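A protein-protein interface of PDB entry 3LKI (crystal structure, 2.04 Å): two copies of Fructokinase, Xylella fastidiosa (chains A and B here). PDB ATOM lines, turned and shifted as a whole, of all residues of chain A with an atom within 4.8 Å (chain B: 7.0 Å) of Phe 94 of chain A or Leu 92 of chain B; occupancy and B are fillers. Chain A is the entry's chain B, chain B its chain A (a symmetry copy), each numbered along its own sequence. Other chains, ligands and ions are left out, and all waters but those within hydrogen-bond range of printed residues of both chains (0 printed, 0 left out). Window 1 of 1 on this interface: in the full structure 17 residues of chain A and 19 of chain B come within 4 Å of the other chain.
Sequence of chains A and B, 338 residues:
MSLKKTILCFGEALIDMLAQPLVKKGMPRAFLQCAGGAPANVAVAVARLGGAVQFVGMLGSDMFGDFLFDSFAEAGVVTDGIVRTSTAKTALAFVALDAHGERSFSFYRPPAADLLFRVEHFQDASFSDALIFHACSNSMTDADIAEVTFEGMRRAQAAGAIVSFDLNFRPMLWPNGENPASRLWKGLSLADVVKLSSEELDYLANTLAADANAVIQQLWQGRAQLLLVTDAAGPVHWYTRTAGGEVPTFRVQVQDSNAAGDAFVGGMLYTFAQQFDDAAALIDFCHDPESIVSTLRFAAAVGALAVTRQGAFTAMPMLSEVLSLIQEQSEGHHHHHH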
ATOM      1  N   MET A  17      27.741  11.585 -25.900  1.00  0.00           N
ATOM      2  CA  MET A  17      26.370  11.788 -26.370  1.00  0.00           C
ATOM      3  C   MET A  17      26.466  12.448 -27.741  1.00  0.00           C
ATOM      4  O   MET A  17      26.765  13.641 -27.857  1.00  0.00           O
ATOM      5  CB  MET A  17      25.586  12.687 -25.411  1.00  0.00           C
ATOM      6  CG  MET A  17      25.284  12.066 -24.050  1.00  0.00           C
ATOM      7  SD  MET A  17      23.939  10.661 -24.116  1.00  0.00           S
ATOM      8  CE  MET A  17      22.361  11.744 -24.022  1.00  0.00           C
ATOM      9  N   PHE A  31      19.914  12.320 -29.217  1.00  0.00           N
ATOM     10  CA  PHE A  31      21.303  12.175 -28.816  1.00  0.00           C
ATOM     11  C   PHE A  31      21.534  10.688 -28.581  1.00  0.00           C
ATOM     12  O   PHE A  31      20.774  10.047 -27.856  1.00  0.00           O
ATOM     13  CB  PHE A  31      21.564  12.965 -27.538  1.00  0.00           C
ATOM     14  CG  PHE A  31      21.624  14.454 -27.747  1.00  0.00           C
ATOM     15  CD1 PHE A  31      22.830  15.078 -28.049  1.00  0.00           C
ATOM     16  CD2 PHE A  31      20.477  15.232 -27.645  1.00  0.00           C
ATOM     17  CE1 PHE A  31      22.897  16.453 -28.243  1.00  0.00           C
ATOM     18  CE2 PHE A  31      20.535  16.617 -27.838  1.00  0.00           C
ATOM     19  CZ  PHE A  31      21.750  17.223 -28.138  1.00  0.00           C
ATOM     20  N   LEU A  92      29.830  13.321 -18.961  1.00  0.00           N
ATOM     21  CA  LEU A  92      29.149  13.298 -20.248  1.00  0.00           C
ATOM     22  C   LEU A  92      29.890  14.200 -21.218  1.00  0.00           C
ATOM     23  O   LEU A  92      30.309  15.303 -20.862  1.00  0.00           O
ATOM     24  CB  LEU A  92      27.706  13.794 -20.118  1.00  0.00           C
ATOM     25  CG  LEU A  92      26.701  13.012 -19.267  1.00  0.00           C
ATOM     26  CD1 LEU A  92      25.348  13.744 -19.290  1.00  0.00           C
ATOM     27  CD2 LEU A  92      26.558  11.590 -19.798  1.00  0.00           C
ATOM     28  N   ALA A  93      30.055  13.721 -22.443  1.00  0.00           N
ATOM     29  CA  ALA A  93      30.721  14.495 -23.474  1.00  0.00           C
ATOM     30  C   ALA A  93      29.757  14.620 -24.655  1.00  0.00           C
ATOM     31  O   ALA A  93      29.573  13.675 -25.429  1.00  0.00           O
ATOM     32  CB  ALA A  93      32.005  13.805 -23.903  1.00  0.00           C
ATOM     33  N   PHE A  94      29.125  15.782 -24.770  1.00  0.00           N
ATOM     34  CA  PHE A  94      28.178  16.029 -25.848  1.00  0.00           C
ATOM     35  C   PHE A  94      28.924  16.427 -27.118  1.00  0.00           C
ATOM     36  O   PHE A  94      29.756  17.333 -27.106  1.00  0.00           O
ATOM     37  CB  PHE A  94      27.180  17.123 -25.437  1.00  0.00           C
ATOM     38  CG  PHE A  94      26.100  16.641 -24.506  1.00  0.00           C
ATOM     39  CD1 PHE A  94      24.951  16.041 -25.003  1.00  0.00           C
ATOM     40  CD2 PHE A  94      26.263  16.730 -23.131  1.00  0.00           C
ATOM     41  CE1 PHE A  94      23.986  15.533 -24.147  1.00  0.00           C
ATOM     42  CE2 PHE A  94      25.306  16.225 -22.267  1.00  0.00           C
ATOM     43  CZ  PHE A  94      24.161  15.622 -22.778  1.00  0.00           C
ATOM     44  N   VAL A  95      28.637  15.730 -28.210  1.00  0.00           N
ATOM     45  CA  VAL A  95      29.282  16.021 -29.483  1.00  0.00           C
ATOM     46  C   VAL A  95      28.229  16.418 -30.515  1.00  0.00           C
ATOM     47  O   VAL A  95      27.294  15.666 -30.785  1.00  0.00           O
ATOM     48  CB  VAL A  95      30.057  14.794 -29.999  1.00  0.00           C
ATOM     49  CG1 VAL A  95      30.862  15.174 -31.231  1.00  0.00           C
ATOM     50  CG2 VAL A  95      30.971  14.260 -28.904  1.00  0.00           C
ATOM     51  N   ALA A  96      28.379  17.608 -31.079  1.00  0.00           N
ATOM     52  CA  ALA A  96      27.444  18.101 -32.078  1.00  0.00           C
ATOM     53  C   ALA A  96      28.186  18.879 -33.147  1.00  0.00           C
ATOM     54  O   ALA A  96      29.380  18.655 -33.379  1.00  0.00           O
ATOM     55  CB  ALA A  96      26.394  18.986 -31.424  1.00  0.00           C
ATOM     56  N   SER A 104      31.680  20.181 -32.646  1.00  0.00           N
ATOM     57  CA  SER A 104      31.702  20.904 -31.379  1.00  0.00           C
ATOM     58  C   SER A 104      31.764  19.985 -30.150  1.00  0.00           C
ATOM     59  O   SER A 104      31.629  18.764 -30.265  1.00  0.00           O
ATOM     60  CB  SER A 104      30.468  21.813 -31.301  1.00  0.00           C
ATOM     61  OG  SER A 104      30.556  22.715 -30.214  1.00  0.00           O
ATOM     62  N   PHE A 105      31.961  20.584 -28.976  1.00  0.00           N
ATOM     63  CA  PHE A 105      32.054  19.834 -27.724  1.00  0.00           C
ATOM     64  C   PHE A 105      31.501  20.582 -26.510  1.00  0.00           C
ATOM     65  O   PHE A 105      31.604  21.809 -26.407  1.00  0.00           O
ATOM     66  CB  PHE A 105      33.510  19.454 -27.442  1.00  0.00           C
ATOM     67  CG  PHE A 105      34.023  18.323 -28.287  1.00  0.00           C
ATOM     68  CD1 PHE A 105      33.695  17.005 -27.984  1.00  0.00           C
ATOM     69  CD2 PHE A 105      34.835  18.573 -29.390  1.00  0.00           C
ATOM     70  CE1 PHE A 105      34.168  15.950 -28.763  1.00  0.00           C
ATOM     71  CE2 PHE A 105      35.314  17.524 -30.180  1.00  0.00           C
ATOM     72  CZ  PHE A 105      34.980  16.213 -29.864  1.00  0.00           C
ATOM     73  N   SER A 106      30.913  19.819 -25.593  1.00  0.00           N
ATOM     74  CA  SER A 106      30.358  20.347 -24.355  1.00  0.00           C
ATOM     75  C   SER A 106      30.466  19.222 -23.329  1.00  0.00           C
ATOM     76  O   SER A 106      29.779  18.205 -23.427  1.00  0.00           O
ATOM     77  CB  SER A 106      28.896  20.758 -24.544  1.00  0.00           C
ATOM     78  OG  SER A 106      28.395  21.371 -23.367  1.00  0.00           O
ATOM     79  N   TYR A 108      30.469  17.631 -19.318  1.00  0.00           N
ATOM     80  CA  TYR A 108      29.897  17.753 -17.986  1.00  0.00           C
ATOM     81  C   TYR A 108      30.956  17.081 -17.108  1.00  0.00           C
ATOM     82  O   TYR A 108      30.825  15.926 -16.711  1.00  0.00           O
ATOM     83  CB  TYR A 108      28.533  17.050 -17.912  1.00  0.00           C
ATOM     84  CG  TYR A 108      27.419  17.935 -18.439  1.00  0.00           C
ATOM     85  CD1 TYR A 108      26.528  18.573 -17.565  1.00  0.00           C
ATOM     86  CD2 TYR A 108      27.312  18.209 -19.801  1.00  0.00           C
ATOM     87  CE1 TYR A 108      25.567  19.466 -18.044  1.00  0.00           C
ATOM     88  CE2 TYR A 108      26.353  19.101 -20.291  1.00  0.00           C
ATOM     89  CZ  TYR A 108      25.490  19.727 -19.409  1.00  0.00           C
ATOM     90  OH  TYR A 108      24.572  20.625 -19.899  1.00  0.00           O
ATOM     91  N   LEU B  14      15.802  24.150 -17.829  1.00  0.00           N
ATOM     92  CA  LEU B  14      16.811  23.128 -18.061  1.00  0.00           C
ATOM     93  C   LEU B  14      16.356  22.188 -19.156  1.00  0.00           C
ATOM     94  O   LEU B  14      15.245  22.321 -19.678  1.00  0.00           O
ATOM     95  CB  LEU B  14      17.104  22.344 -16.768  1.00  0.00           C
ATOM     96  CG  LEU B  14      16.198  21.268 -16.141  1.00  0.00           C
ATOM     97  CD1 LEU B  14      16.041  21.576 -14.663  1.00  0.00           C
ATOM     98  CD2 LEU B  14      14.845  21.187 -16.799  1.00  0.00           C
ATOM     99  N   ILE B  15      17.217  21.239 -19.493  1.00  0.00           N
ATOM    100  CA  ILE B  15      16.914  20.274 -20.538  1.00  0.00           C
ATOM    101  C   ILE B  15      16.451  18.941 -19.977  1.00  0.00           C
ATOM    102  O   ILE B  15      17.100  18.360 -19.109  1.00  0.00           O
ATOM    103  CB  ILE B  15      18.153  19.990 -21.421  1.00  0.00           C
ATOM    104  CG1 ILE B  15      18.679  21.287 -22.045  1.00  0.00           C
ATOM    105  CG2 ILE B  15      17.793  18.977 -22.494  1.00  0.00           C
ATOM    106  CD1 ILE B  15      17.718  21.963 -22.997  1.00  0.00           C
ATOM    107  N   ASP B  16      15.309  18.477 -20.460  1.00  0.00           N
ATOM    108  CA  ASP B  16      14.779  17.179 -20.068  1.00  0.00           C
ATOM    109  C   ASP B  16      15.262  16.225 -21.165  1.00  0.00           C
ATOM    110  O   ASP B  16      14.970  16.426 -22.342  1.00  0.00           O
ATOM    111  CB  ASP B  16      13.244  17.202 -20.030  1.00  0.00           C
ATOM    112  CG  ASP B  16      12.692  17.810 -18.744  1.00  0.00           C
ATOM    113  OD1 ASP B  16      11.582  18.376 -18.778  1.00  0.00           O
ATOM    114  OD2 ASP B  16      13.355  17.708 -17.692  1.00  0.00           O
ATOM    115  N   MET B  17      16.039  15.220 -20.784  1.00  0.00           N
ATOM    116  CA  MET B  17      16.527  14.242 -21.743  1.00  0.00           C
ATOM    117  C   MET B  17      15.737  12.956 -21.519  1.00  0.00           C
ATOM    118  O   MET B  17      15.916  12.264 -20.511  1.00  0.00           O
ATOM    119  CB  MET B  17      18.027  14.016 -21.553  1.00  0.00           C
ATOM    120  CG  MET B  17      18.897  15.203 -21.961  1.00  0.00           C
ATOM    121  SD  MET B  17      19.098  15.434 -23.871  1.00  0.00           S
ATOM    122  CE  MET B  17      20.567  14.260 -24.201  1.00  0.00           C
ATOM    123  N   MET B  63      25.283  24.900 -25.813  1.00  0.00           N
ATOM    124  CA  MET B  63      24.309  24.541 -26.850  1.00  0.00           C
ATOM    125  C   MET B  63      22.906  24.452 -26.279  1.00  0.00           C
ATOM    126  O   MET B  63      21.946  24.930 -26.881  1.00  0.00           O
ATOM    127  CB  MET B  63      24.684  23.196 -27.541  1.00  0.00           C
ATOM    128  CG  MET B  63      24.621  21.911 -26.663  1.00  0.00           C
ATOM    129  SD  MET B  63      25.314  20.244 -27.557  1.00  0.00           S
ATOM    130  CE  MET B  63      27.121  20.873 -27.874  1.00  0.00           C
ATOM    131  N   PHE B  64      22.793  23.852 -25.103  1.00  0.00           N
ATOM    132  CA  PHE B  64      21.498  23.711 -24.468  1.00  0.00           C
ATOM    133  C   PHE B  64      20.911  25.069 -24.063  1.00  0.00           C
ATOM    134  O   PHE B  64      19.711  25.307 -24.233  1.00  0.00           O
ATOM    135  CB  PHE B  64      21.626  22.775 -23.274  1.00  0.00           C
ATOM    136  CG  PHE B  64      22.040  21.377 -23.652  1.00  0.00           C
ATOM    137  CD1 PHE B  64      21.262  20.621 -24.528  1.00  0.00           C
ATOM    138  CD2 PHE B  64      23.199  20.814 -23.133  1.00  0.00           C
ATOM    139  CE1 PHE B  64      21.628  19.321 -24.877  1.00  0.00           C
ATOM    140  CE2 PHE B  64      23.576  19.511 -23.474  1.00  0.00           C
ATOM    141  CZ  PHE B  64      22.789  18.764 -24.348  1.00  0.00           C
ATOM    142  N   LYS B  89      27.318  24.588 -16.721  1.00  0.00           N
ATOM    143  CA  LYS B  89      26.518  24.079 -17.823  1.00  0.00           C
ATOM    144  C   LYS B  89      25.032  24.067 -17.495  1.00  0.00           C
ATOM    145  O   LYS B  89      24.629  23.955 -16.335  1.00  0.00           O
ATOM    146  CB  LYS B  89      26.948  22.651 -18.168  1.00  0.00           C
ATOM    147  CG  LYS B  89      28.409  22.493 -18.561  1.00  0.00           C
ATOM    148  CD  LYS B  89      28.702  23.207 -19.867  1.00  0.00           C
ATOM    149  CE  LYS B  89      30.163  23.040 -20.276  1.00  0.00           C
ATOM    150  NZ  LYS B  89      30.395  23.601 -21.639  1.00  0.00           N
ATOM    151  N   THR B  90      24.221  24.177 -18.535  1.00  0.00           N
ATOM    152  CA  THR B  90      22.779  24.145 -18.384  1.00  0.00           C
ATOM    153  C   THR B  90      22.454  22.805 -17.739  1.00  0.00           C
ATOM    154  O   THR B  90      23.005  21.778 -18.135  1.00  0.00           O
ATOM    155  CB  THR B  90      22.110  24.255 -19.755  1.00  0.00           C
ATOM    156  OG1 THR B  90      22.434  25.529 -20.335  1.00  0.00           O
ATOM    157  CG2 THR B  90      20.603  24.105 -19.634  1.00  0.00           C
ATOM    158  N   ALA B  91      21.587  22.811 -16.734  1.00  0.00           N
ATOM    159  CA  ALA B  91      21.250  21.569 -16.051  1.00  0.00           C
ATOM    160  C   ALA B  91      20.561  20.562 -16.966  1.00  0.00           C
ATOM    161  O   ALA B  91      19.918  20.934 -17.949  1.00  0.00           O
ATOM    162  CB  ALA B  91      20.376  21.856 -14.835  1.00  0.00           C
ATOM    163  N   LEU B  92      20.713  19.284 -16.637  1.00  0.00           N
ATOM    164  CA  LEU B  92      20.120  18.201 -17.412  1.00  0.00           C
ATOM    165  C   LEU B  92      19.267  17.305 -16.535  1.00  0.00           C
ATOM    166  O   LEU B  92      19.656  16.955 -15.422  1.00  0.00           O
ATOM    167  CB  LEU B  92      21.209  17.352 -18.077  1.00  0.00           C
ATOM    168  CG  LEU B  92      22.176  18.082 -19.009  1.00  0.00           C
ATOM    169  CD1 LEU B  92      23.182  17.085 -19.589  1.00  0.00           C
ATOM    170  CD2 LEU B  92      21.388  18.769 -20.119  1.00  0.00           C
ATOM    171  N   ALA B  93      18.103  16.934 -17.050  1.00  0.00           N
ATOM    172  CA  ALA B  93      17.187  16.065 -16.333  1.00  0.00           C
ATOM    173  C   ALA B  93      16.967  14.803 -17.162  1.00  0.00           C
ATOM    174  O   ALA B  93      16.167  14.799 -18.094  1.00  0.00           O
ATOM    175  CB  ALA B  93      15.869  16.779 -16.112  1.00  0.00           C
ATOM    176  N   PHE B  94      17.696  13.744 -16.823  1.00  0.00           N
ATOM    177  CA  PHE B  94      17.576  12.474 -17.525  1.00  0.00           C
ATOM    178  C   PHE B  94      16.483  11.614 -16.902  1.00  0.00           C
ATOM    179  O   PHE B  94      16.435  11.431 -15.687  1.00  0.00           O
ATOM    180  CB  PHE B  94      18.899  11.701 -17.474  1.00  0.00           C
ATOM    181  CG  PHE B  94      19.939  12.214 -18.422  1.00  0.00           C
ATOM    182  CD1 PHE B  94      19.929  11.829 -19.761  1.00  0.00           C
ATOM    183  CD2 PHE B  94      20.919  13.096 -17.985  1.00  0.00           C
ATOM    184  CE1 PHE B  94      20.878  12.305 -20.643  1.00  0.00           C
ATOM    185  CE2 PHE B  94      21.876  13.581 -18.862  1.00  0.00           C
ATOM    186  CZ  PHE B  94      21.854  13.183 -20.198  1.00  0.00           C
ATOM    187  N   SER B 106      18.120  11.062 -13.218  1.00  0.00           N
ATOM    188  CA  SER B 106      19.514  11.427 -13.050  1.00  0.00           C
ATOM    189  C   SER B 106      19.626  12.907 -13.365  1.00  0.00           C
ATOM    190  O   SER B 106      19.490  13.326 -14.513  1.00  0.00           O
ATOM    191  CB  SER B 106      20.418  10.625 -13.983  1.00  0.00           C
ATOM    192  OG  SER B 106      21.772  10.869 -13.651  1.00  0.00           O
ATOM    193  N   PHE B 107      19.862  13.703 -12.337  1.00  0.00           N
ATOM    194  CA  PHE B 107      19.968  15.135 -12.517  1.00  0.00           C
ATOM    195  C   PHE B 107      21.411  15.613 -12.491  1.00  0.00           C
ATOM    196  O   PHE B 107      22.182  15.229 -11.614  1.00  0.00           O
ATOM    197  CB  PHE B 107      19.171  15.848 -11.423  1.00  0.00           C
ATOM    198  CG  PHE B 107      17.690  15.607 -11.495  1.00  0.00           C
ATOM    199  CD1 PHE B 107      16.898  16.317 -12.391  1.00  0.00           C
ATOM    200  CD2 PHE B 107      17.090  14.648 -10.685  1.00  0.00           C
ATOM    201  CE1 PHE B 107      15.528  16.077 -12.481  1.00  0.00           C
ATOM    202  CE2 PHE B 107      15.724  14.400 -10.769  1.00  0.00           C
ATOM    203  CZ  PHE B 107      14.939  15.116 -11.671  1.00  0.00           C
ATOM    204  N   TYR B 108      21.776  16.422 -13.478  1.00  0.00           N
ATOM    205  CA  TYR B 108      23.108  17.012 -13.536  1.00  0.00           C
ATOM    206  C   TYR B 108      22.867  18.431 -13.041  1.00  0.00           C
ATOM    207  O   TYR B 108      22.771  19.380 -13.817  1.00  0.00           O
ATOM    208  CB  TYR B 108      23.653  16.994 -14.968  1.00  0.00           C
ATOM    209  CG  TYR B 108      24.222  15.641 -15.334  1.00  0.00           C
ATOM    210  CD1 TYR B 108      25.603  15.440 -15.424  1.00  0.00           C
ATOM    211  CD2 TYR B 108      23.382  14.535 -15.505  1.00  0.00           C
ATOM    212  CE1 TYR B 108      26.130  14.169 -15.665  1.00  0.00           C
ATOM    213  CE2 TYR B 108      23.901  13.266 -15.746  1.00  0.00           C
ATOM    214  CZ  TYR B 108      25.277  13.087 -15.821  1.00  0.00           C
ATOM    215  OH  TYR B 108      25.780  11.823 -16.013  1.00  0.00           O
ATOM    216  N   ARG B 109      22.739  18.527 -11.722  1.00  0.00           N
ATOM    217  CA  ARG B 109      22.446  19.766 -11.009  1.00  0.00           C
ATOM    218  C   ARG B 109      22.361  19.370  -9.536  1.00  0.00           C
ATOM    219  O   ARG B 109      21.563  18.509  -9.172  1.00  0.00           O
ATOM    220  CB  ARG B 109      21.084  20.307 -11.470  1.00  0.00           C
ATOM    221  CG  ARG B 109      20.546  21.525 -10.713  1.00  0.00           C
ATOM    222  CD  ARG B 109      19.185  21.894 -11.287  1.00  0.00           C
ATOM    223  NE  ARG B 109      18.713  23.210 -10.872  1.00  0.00           N
ATOM    224  CZ  ARG B 109      18.124  23.474  -9.709  1.00  0.00           C
ATOM    225  NH1 ARG B 109      17.930  22.507  -8.822  1.00  0.00           N
ATOM    226  NH2 ARG B 109      17.726  24.708  -9.438  1.00  0.00           N
ATOM    227  N   PRO B 111      26.414  21.064 -10.035  1.00  0.00           N
ATOM    228  CA  PRO B 111      26.262  22.495 -10.314  1.00  0.00           C
ATOM    229  C   PRO B 111      25.415  22.701 -11.570  1.00  0.00           C
ATOM    230  O   PRO B 111      25.122  21.741 -12.279  1.00  0.00           O
ATOM    231  CB  PRO B 111      27.701  22.952 -10.515  1.00  0.00           C
ATOM    232  CG  PRO B 111      28.307  21.756 -11.223  1.00  0.00           C
ATOM    233  CD  PRO B 111      27.775  20.606 -10.379  1.00  0.00           C
ATOM    234  N   ALA B 112      25.044  23.952 -11.844  1.00  0.00           N
ATOM    235  CA  ALA B 112      24.237  24.295 -13.009  1.00  0.00           C
ATOM    236  C   ALA B 112      24.132  25.811 -13.193  1.00  0.00           C
ATOM    237  O   ALA B 112      24.148  26.575 -12.224  1.00  0.00           O
ATOM    238  CB  ALA B 112      22.834  23.691 -12.878  1.00  0.00           C
ATOM    239  N   LEU B 173      16.132  16.705  -6.075  1.00  0.00           N
ATOM    240  CA  LEU B 173      16.979  17.843  -6.424  1.00  0.00           C
ATOM    241  C   LEU B 173      17.637  18.481  -5.205  1.00  0.00           C
ATOM    242  O   LEU B 173      18.498  19.354  -5.337  1.00  0.00           O
ATOM    243  CB  LEU B 173      16.165  18.909  -7.172  1.00  0.00           C
ATOM    244  CG  LEU B 173      15.692  18.591  -8.595  1.00  0.00           C
ATOM    245  CD1 LEU B 173      14.876  19.765  -9.141  1.00  0.00           C
ATOM    246  CD2 LEU B 173      16.898  18.326  -9.486  1.00  0.00           C
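The side-chain amino group (NZ) of Lys 89 of chain B lies within hydrogen-bond range of the side-chain hydroxyl (OG) of Ser 106 of chain A, at 3.5 Å. O of Thr 90 of chain B sits at hydrogen-bond distance from OH of Tyr 108 of chain A, at 2.6 Å.
The backbone NH of Met 17 of chain A is in hydrogen-bond range of the backbone carbonyl oxygen of Ala 93 of chain A, at 2.8 Å. The backbone carbonyl oxygen (O) of Met 17 of chain A is in hydrogen-bond range of the backbone NH (N) of Val 95 of chain A. O of Leu 92 of chain A lies within hydrogen-bond range of N of Tyr 108 of chain A, 2.8 Å away. The backbone NH (N) of Phe 94 of chain A lies within hydrogen-bond range of the backbone carbonyl oxygen (O) of Ser 106 of chain A (2.8 Å). N of Tyr 108 of chain B is in hydrogen-bond range of O of Leu 92 of chain B, 2.9 Å away. N of Phe 94 of chain B lies within hydrogen-bond range of O of Ser 106 of chain B, 3.0 Å away.
Among the printed residues, pairs that only touch across the chains: Met 17 of chain A with Met 17 of chain B, Met 17 of chain A with Phe 94 of chain B, Phe 31 of chain A with Met 17 of chain B, Phe 31 of chain A with Phe 64 of chain B, Leu 92 of chain A with Leu 92 of chain B, Leu 92 of chain A with Phe 94 of chain B, Leu 92 of chain A with Tyr 108 of chain B, Phe 94 of chain A with Met 17 of chain B, Phe 94 of chain A with Phe 64 of chain B, Phe 94 of chain A with Leu 92 of chain B, Ser 106 of chain A with Met 63 of chain B, Tyr 108 of chain A with Phe 64 of chain B, Tyr 108 of chain A with Lys 89 of chain B, Tyr 108 of chain A with Leu 92 of chain B and Tyr 108 of chain A with Tyr 108 of chain B.
Printed residues of chain B within 4 Å of Met 17 of chain A: Met 17 and Phe 94. Of the printed residues of chain B, Phe 31 of chain A touches Met 17 and Phe 64. Of the printed residues of chain B, Ser 106 of chain A touches Met 63 (3.8 Å) and Lys 89 (3.5 Å). Of the printed residues of chain A, Met 17 of chain B touches Met 17 (3.1 Å), Phe 31 (3.6 Å) and Phe 94 (3.6 Å). Of the printed residues of chain A, Met 63 of chain B touches Ser 106. Printed residues of chain A within 4 Å of Leu 92 of chain B: Leu 92, Phe 94 and Tyr 108. Ser 106 of chain B touches none of the printed residues of chain A.
Hydrophobic or aromatic side chains of chain A that line the printed part of chain B: Met 17, Phe 31, Leu 92, Phe 94 and Tyr 108. Hydrophobic or aromatic side chains of chain B within 4 Å of the printed part of chain A: Met 17, Met 63, Phe 64, Leu 92, Phe 94 and Tyr 108. Among the printed residues, no Asp or Glu carboxylate lies within 4 Å of a Lys or Arg side-chain nitrogen of the other chain.
Met 17 of chain B touches its own counterpart, Met 17 of chain A. Leu 92 of chain B touches its own counterpart, Leu 92 of chain A. Leu 92 of chain A touches Tyr 108 of chain B, and with the chains exchanged Tyr 108 of chain A touches Leu 92 of chain B. Tyr 108 of chain A touches its own counterpart, Tyr 108 of chain B. 6 positions are printed for both chains. Of the 17 pairs that touch across the chains among the printed residues, 9 have their exchanged pair printed and touching as well.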
